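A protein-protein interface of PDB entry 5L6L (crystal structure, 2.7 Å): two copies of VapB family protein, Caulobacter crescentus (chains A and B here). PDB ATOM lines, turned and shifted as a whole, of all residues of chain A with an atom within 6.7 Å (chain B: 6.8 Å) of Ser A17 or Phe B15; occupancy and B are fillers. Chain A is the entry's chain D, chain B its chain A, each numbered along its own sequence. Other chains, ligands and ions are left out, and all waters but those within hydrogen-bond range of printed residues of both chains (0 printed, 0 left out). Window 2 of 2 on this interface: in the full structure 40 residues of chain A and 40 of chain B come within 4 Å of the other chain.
O of Gly A32 sits close to OE1 of Glu B21. The backbone NH (N) of Val B23 is in hydrogen-bond range of the backbone carbonyl oxygen (O) of Val A23, 2.9 Å away. The side-chain hydroxyl (OG1) of Thr B14 is in hydrogen-bond range of the backbone carbonyl oxygen (O) of Gly A32.
O of Phe A15 is in hydrogen-bond range of N of Ala A22. The guanidinium group of Arg A16 is in salt-bridge range of the side-chain carboxylate of Glu A21 (3.9 Å). The backbone carbonyl oxygen (O) of Phe B15 lies within hydrogen-bond range of the backbone NH (N) of Ala B22 (3.1 Å). NH1 of Arg B16 lies within salt-bridge range of OE1 of Glu B21 (3.9 Å).
Phe A15 touches Ser B17 (CE2 to OG, 3.7 Å). Phe A15 touches Ala B22 (CZ to CB, 3.96 Å). Phe B15 touches Ser A17 (CE2 to OG, 3.7 Å). Arg B24 touches Glu A21 (CA to O, 3.4 Å). CA of Ala A22 touches O of Val B23, 3.3 Å away. Ala B22 touches Val A23. Thr B14 touches Asp A34 (OG1 to N, 3.6 Å). Leu A37 touches Thr B14. Val B23 touches Leu A37.
Of chain B, only Phe B15 comes within 4 Å of Ser A17. Of chain A, only Ser A17 (3.7 Å) comes within 4 Å of Phe B15. Of the printed residues of chain A, Arg B24 touches Glu A21 (3.4 Å). Of the printed residues of chain A, Ala B22 touches Phe A15 (3.96 Å) and Val A23 (3.2 Å). Printed residues of chain A within 4 Å of Ser B17: Phe A15. Of the printed residues of chain B, Asp A34 touches Thr B14.
Hydrophobic or aromatic side chains of chain A that line the printed part of chain B: Phe A15, Ala A22, Val A23 and Leu A37. Among the printed residues, 12 pairs touch across the chains.
Phe A15 touches Ser B17, and with the chains exchanged Ser A17 touches Phe B15. Phe A15 touches Ala B22, but with the chains exchanged Ala A22 does not touch Phe B15 (4.4 Å). Ala A22 touches Val B23, and with the chains exchanged Val A23 touches Ala B22. Val B23 touches its own counterpart, Val A23. Positions printed for both chains: 15, 16, 17, 18, 20, 21, 22 and 23.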
ATOM      1  N   PHE A  15      22.346  20.291   4.276  1.00  0.00           N
ATOM      2  CA  PHE A  15      22.479  19.349   5.376  1.00  0.00           C
ATOM      3  C   PHE A  15      21.138  19.293   6.097  1.00  0.00           C
ATOM      4  O   PHE A  15      20.313  20.209   5.988  1.00  0.00           O
ATOM      5  CB  PHE A  15      23.611  19.751   6.333  1.00  0.00           C
ATOM      6  CG  PHE A  15      23.290  20.947   7.184  1.00  0.00           C
ATOM      7  CD1 PHE A  15      23.280  22.216   6.646  1.00  0.00           C
ATOM      8  CD2 PHE A  15      22.995  20.797   8.526  1.00  0.00           C
ATOM      9  CE1 PHE A  15      22.977  23.315   7.431  1.00  0.00           C
ATOM     10  CE2 PHE A  15      22.696  21.886   9.309  1.00  0.00           C
ATOM     11  CZ  PHE A  15      22.687  23.146   8.764  1.00  0.00           C
ATOM     12  N   ARG A  16      20.912  18.205   6.827  1.00  0.00           N
ATOM     13  CA  ARG A  16      19.668  18.029   7.566  1.00  0.00           C
ATOM     14  C   ARG A  16      19.869  18.495   9.000  1.00  0.00           C
ATOM     15  O   ARG A  16      20.923  18.265   9.600  1.00  0.00           O
ATOM     16  CB  ARG A  16      19.194  16.572   7.507  1.00  0.00           C
ATOM     17  CG  ARG A  16      19.201  16.046   6.073  1.00  0.00           C
ATOM     18  CD  ARG A  16      17.949  15.298   5.658  1.00  0.00           C
ATOM     19  NE  ARG A  16      16.706  15.882   6.158  1.00  0.00           N
ATOM     20  CZ  ARG A  16      15.844  16.576   5.421  1.00  0.00           C
ATOM     21  NH1 ARG A  16      16.087  16.802   4.142  1.00  0.00           N
ATOM     22  NH2 ARG A  16      14.732  17.045   5.965  1.00  0.00           N
ATOM     23  N   SER A  17      18.873  19.200   9.524  1.00  0.00           N
ATOM     24  CA  SER A  17      18.890  19.716  10.889  1.00  0.00           C
ATOM     25  C   SER A  17      17.542  19.372  11.487  1.00  0.00           C
ATOM     26  O   SER A  17      16.529  19.953  11.097  1.00  0.00           O
ATOM     27  CB  SER A  17      19.131  21.227  10.924  1.00  0.00           C
ATOM     28  OG  SER A  17      18.923  21.749  12.228  1.00  0.00           O
ATOM     29  N   GLY A  18      17.525  18.430  12.422  1.00  0.00           N
ATOM     30  CA  GLY A  18      16.250  17.905  12.870  1.00  0.00           C
ATOM     31  C   GLY A  18      15.542  17.282  11.690  1.00  0.00           C
ATOM     32  O   GLY A  18      16.118  16.486  10.935  1.00  0.00           O
ATOM     33  N   ASN A  19      14.293  17.682  11.484  1.00  0.00           N
ATOM     34  CA  ASN A  19      13.482  17.061  10.450  1.00  0.00           C
ATOM     35  C   ASN A  19      13.389  17.882   9.158  1.00  0.00           C
ATOM     36  O   ASN A  19      12.895  17.361   8.154  1.00  0.00           O
ATOM     37  CB  ASN A  19      12.078  16.759  11.008  1.00  0.00           C
ATOM     38  CG  ASN A  19      12.104  15.758  12.192  1.00  0.00           C
ATOM     39  OD1 ASN A  19      12.771  14.721  12.145  1.00  0.00           O
ATOM     40  ND2 ASN A  19      11.368  16.081  13.256  1.00  0.00           N
ATOM     41  N   SER A  20      13.875  19.122   9.133  1.00  0.00           N
ATOM     42  CA  SER A  20      13.886  19.926   7.915  1.00  0.00           C
ATOM     43  C   SER A  20      15.247  19.883   7.237  1.00  0.00           C
ATOM     44  O   SER A  20      16.222  19.368   7.774  1.00  0.00           O
ATOM     45  CB  SER A  20      13.515  21.379   8.212  1.00  0.00           C
ATOM     46  OG  SER A  20      12.220  21.466   8.765  1.00  0.00           O
ATOM     47  N   GLU A  21      15.304  20.451   6.039  1.00  0.00           N
ATOM     48  CA  GLU A  21      16.560  20.669   5.329  1.00  0.00           C
ATOM     49  C   GLU A  21      17.090  22.068   5.639  1.00  0.00           C
ATOM     50  O   GLU A  21      16.340  22.971   6.021  1.00  0.00           O
ATOM     51  CB  GLU A  21      16.352  20.486   3.824  1.00  0.00           C
ATOM     52  CG  GLU A  21      17.597  20.540   2.952  1.00  0.00           C
ATOM     53  CD  GLU A  21      17.260  20.346   1.483  1.00  0.00           C
ATOM     54  OE1 GLU A  21      17.404  21.301   0.683  1.00  0.00           O
ATOM     55  OE2 GLU A  21      16.813  19.235   1.134  1.00  0.00           O
ATOM     56  N   ALA A  22      18.400  22.246   5.493  1.00  0.00           N
ATOM     57  CA  ALA A  22      18.957  23.547   5.824  1.00  0.00           C
ATOM     58  C   ALA A  22      20.208  23.811   5.012  1.00  0.00           C
ATOM     59  O   ALA A  22      20.855  22.890   4.506  1.00  0.00           O
ATOM     60  CB  ALA A  22      19.289  23.673   7.309  1.00  0.00           C
ATOM     61  N   VAL A  23      20.529  25.100   4.902  1.00  0.00           N
ATOM     62  CA  VAL A  23      21.759  25.598   4.303  1.00  0.00           C
ATOM     63  C   VAL A  23      22.497  26.386   5.369  1.00  0.00           C
ATOM     64  O   VAL A  23      21.887  27.195   6.075  1.00  0.00           O
ATOM     65  CB  VAL A  23      21.476  26.482   3.078  1.00  0.00           C
ATOM     66  CG1 VAL A  23      20.995  25.627   1.920  1.00  0.00           C
ATOM     67  CG2 VAL A  23      20.422  27.516   3.425  1.00  0.00           C
ATOM     68  N   GLY A  32      21.487  38.709  10.145  1.00  0.00           N
ATOM     69  CA  GLY A  32      21.783  38.732  11.567  1.00  0.00           C
ATOM     70  C   GLY A  32      21.275  37.561  12.405  1.00  0.00           C
ATOM     71  O   GLY A  32      20.929  36.502  11.887  1.00  0.00           O
ATOM     72  N   ASP A  34      18.197  36.334  14.937  1.00  0.00           N
ATOM     73  CA  ASP A  34      16.764  36.607  15.065  1.00  0.00           C
ATOM     74  C   ASP A  34      16.276  37.547  13.961  1.00  0.00           C
ATOM     75  O   ASP A  34      15.669  38.587  14.226  1.00  0.00           O
ATOM     76  CB  ASP A  34      16.422  37.207  16.441  1.00  0.00           C
ATOM     77  CG  ASP A  34      17.157  36.541  17.589  1.00  0.00           C
ATOM     78  OD1 ASP A  34      17.125  35.290  17.686  1.00  0.00           O
ATOM     79  OD2 ASP A  34      17.763  37.280  18.404  1.00  0.00           O
ATOM     80  N   LEU A  37      12.872  36.154   7.797  1.00  0.00           N
ATOM     81  CA  LEU A  37      13.244  36.024   6.402  1.00  0.00           C
ATOM     82  C   LEU A  37      12.017  35.737   5.560  1.00  0.00           C
ATOM     83  O   LEU A  37      11.043  35.137   6.026  1.00  0.00           O
ATOM     84  CB  LEU A  37      14.273  34.898   6.205  1.00  0.00           C
ATOM     85  CG  LEU A  37      15.550  35.045   7.046  1.00  0.00           C
ATOM     86  CD1 LEU A  37      16.421  33.797   7.000  1.00  0.00           C
ATOM     87  CD2 LEU A  37      16.320  36.270   6.577  1.00  0.00           C
ATOM     88  N   LYS B  13      13.153  32.161   9.985  1.00  0.00           N
ATOM     89  CA  LYS B  13      14.036  32.906  10.867  1.00  0.00           C
ATOM     90  C   LYS B  13      15.398  32.229  10.846  1.00  0.00           C
ATOM     91  O   LYS B  13      15.484  31.005  10.723  1.00  0.00           O
ATOM     92  CB  LYS B  13      13.430  32.964  12.285  1.00  0.00           C
ATOM     93  CG  LYS B  13      14.177  33.817  13.277  1.00  0.00           C
ATOM     94  CD  LYS B  13      13.263  34.255  14.436  1.00  0.00           C
ATOM     95  CE  LYS B  13      12.842  33.103  15.353  1.00  0.00           C
ATOM     96  NZ  LYS B  13      11.860  33.557  16.393  1.00  0.00           N
ATOM     97  N   THR B  14      16.465  33.026  10.894  1.00  0.00           N
ATOM     98  CA  THR B  14      17.793  32.440  11.042  1.00  0.00           C
ATOM     99  C   THR B  14      17.898  31.726  12.384  1.00  0.00           C
ATOM    100  O   THR B  14      17.192  32.050  13.349  1.00  0.00           O
ATOM    101  CB  THR B  14      18.910  33.497  10.945  1.00  0.00           C
ATOM    102  OG1 THR B  14      18.615  34.635  11.767  1.00  0.00           O
ATOM    103  CG2 THR B  14      19.128  33.953   9.516  1.00  0.00           C
ATOM    104  N   PHE B  15      18.788  30.738  12.437  1.00  0.00           N
ATOM    105  CA  PHE B  15      19.051  30.045  13.688  1.00  0.00           C
ATOM    106  C   PHE B  15      20.522  29.649  13.743  1.00  0.00           C
ATOM    107  O   PHE B  15      21.223  29.660  12.728  1.00  0.00           O
ATOM    108  CB  PHE B  15      18.114  28.839  13.859  1.00  0.00           C
ATOM    109  CG  PHE B  15      18.443  27.641  12.993  1.00  0.00           C
ATOM    110  CD1 PHE B  15      18.059  27.595  11.655  1.00  0.00           C
ATOM    111  CD2 PHE B  15      19.081  26.527  13.538  1.00  0.00           C
ATOM    112  CE1 PHE B  15      18.334  26.475  10.856  1.00  0.00           C
ATOM    113  CE2 PHE B  15      19.362  25.405  12.748  1.00  0.00           C
ATOM    114  CZ  PHE B  15      18.984  25.386  11.398  1.00  0.00           C
ATOM    115  N   ARG B  16      20.993  29.318  14.944  1.00  0.00           N
ATOM    116  CA  ARG B  16      22.380  28.910  15.112  1.00  0.00           C
ATOM    117  C   ARG B  16      22.485  27.388  15.061  1.00  0.00           C
ATOM    118  O   ARG B  16      21.800  26.685  15.807  1.00  0.00           O
ATOM    119  CB  ARG B  16      22.959  29.451  16.421  1.00  0.00           C
ATOM    120  CG  ARG B  16      22.883  30.966  16.590  1.00  0.00           C
ATOM    121  CD  ARG B  16      23.612  31.716  15.490  1.00  0.00           C
ATOM    122  NE  ARG B  16      25.050  31.463  15.480  1.00  0.00           N
ATOM    123  CZ  ARG B  16      25.867  31.861  14.510  1.00  0.00           C
ATOM    124  NH1 ARG B  16      25.383  32.529  13.475  1.00  0.00           N
ATOM    125  NH2 ARG B  16      27.164  31.587  14.574  1.00  0.00           N
ATOM    126  N   SER B  17      23.335  26.884  14.167  1.00  0.00           N
ATOM    127  CA  SER B  17      23.569  25.448  14.056  1.00  0.00           C
ATOM    128  C   SER B  17      25.001  25.108  14.438  1.00  0.00           C
ATOM    129  O   SER B  17      25.749  24.566  13.617  1.00  0.00           O
ATOM    130  CB  SER B  17      23.279  24.960  12.634  1.00  0.00           C
ATOM    131  OG  SER B  17      23.555  23.577  12.495  1.00  0.00           O
ATOM    132  N   GLY B  18      25.377  25.423  15.684  1.00  0.00           N
ATOM    133  CA  GLY B  18      26.738  25.307  16.179  1.00  0.00           C
ATOM    134  C   GLY B  18      27.767  26.112  15.407  1.00  0.00           C
ATOM    135  O   GLY B  18      28.248  25.658  14.367  1.00  0.00           O
ATOM    136  N   SER B  20      27.969  28.223  13.240  1.00  0.00           N
ATOM    137  CA  SER B  20      27.644  28.828  11.961  1.00  0.00           C
ATOM    138  C   SER B  20      26.157  29.064  11.891  1.00  0.00           C
ATOM    139  O   SER B  20      25.368  28.269  12.405  1.00  0.00           O
ATOM    140  CB  SER B  20      28.071  27.976  10.771  1.00  0.00           C
ATOM    141  OG  SER B  20      29.449  28.152  10.501  1.00  0.00           O
ATOM    142  N   GLU B  21      25.786  30.161  11.246  1.00  0.00           N
ATOM    143  CA  GLU B  21      24.387  30.439  11.000  1.00  0.00           C
ATOM    144  C   GLU B  21      23.837  29.441   9.988  1.00  0.00           C
ATOM    145  O   GLU B  21      24.577  28.784   9.257  1.00  0.00           O
ATOM    146  CB  GLU B  21      24.224  31.874  10.511  1.00  0.00           C
ATOM    147  CG  GLU B  21      22.792  32.384  10.497  1.00  0.00           C
ATOM    148  CD  GLU B  21      22.716  33.861  10.159  1.00  0.00           C
ATOM    149  OE1 GLU B  21      23.301  34.663  10.922  1.00  0.00           O
ATOM    150  OE2 GLU B  21      22.090  34.210   9.129  1.00  0.00           O
ATOM    151  N   ALA B  22      22.517  29.314   9.966  1.00  0.00           N
ATOM    152  CA  ALA B  22      21.864  28.434   9.010  1.00  0.00           C
ATOM    153  C   ALA B  22      20.426  28.882   8.845  1.00  0.00           C
ATOM    154  O   ALA B  22      19.855  29.540   9.721  1.00  0.00           O
ATOM    155  CB  ALA B  22      21.913  26.973   9.454  1.00  0.00           C
ATOM    156  N   VAL B  23      19.839  28.493   7.718  1.00  0.00           N
ATOM    157  CA  VAL B  23      18.453  28.808   7.392  1.00  0.00           C
ATOM    158  C   VAL B  23      17.760  27.524   6.972  1.00  0.00           C
ATOM    159  O   VAL B  23      18.310  26.755   6.177  1.00  0.00           O
ATOM    160  CB  VAL B  23      18.358  29.857   6.270  1.00  0.00           C
ATOM    161  CG1 VAL B  23      16.924  30.095   5.889  1.00  0.00           C
ATOM    162  CG2 VAL B  23      18.985  31.137   6.734  1.00  0.00           C
ATOM    163  N   ARG B  24      16.553  27.299   7.498  1.00  0.00           N
ATOM    164  CA  ARG B  24      15.758  26.127   7.137  1.00  0.00           C
ATOM    165  C   ARG B  24      15.041  26.330   5.804  1.00  0.00           C
ATOM    166  O   ARG B  24      14.584  27.430   5.474  1.00  0.00           O
ATOM    167  CB  ARG B  24      14.731  25.814   8.228  1.00  0.00           C
ATOM    168  CG  ARG B  24      15.257  24.965   9.368  1.00  0.00           C
ATOM    169  CD  ARG B  24      14.208  24.777  10.458  1.00  0.00           C
ATOM    170  NE  ARG B  24      14.109  25.976  11.263  1.00  0.00           N
ATOM    171  CZ  ARG B  24      14.756  26.158  12.404  1.00  0.00           C
ATOM    172  NH1 ARG B  24      15.531  25.188  12.896  1.00  0.00           N
ATOM    173  NH2 ARG B  24      14.616  27.308  13.060  1.00  0.00           N
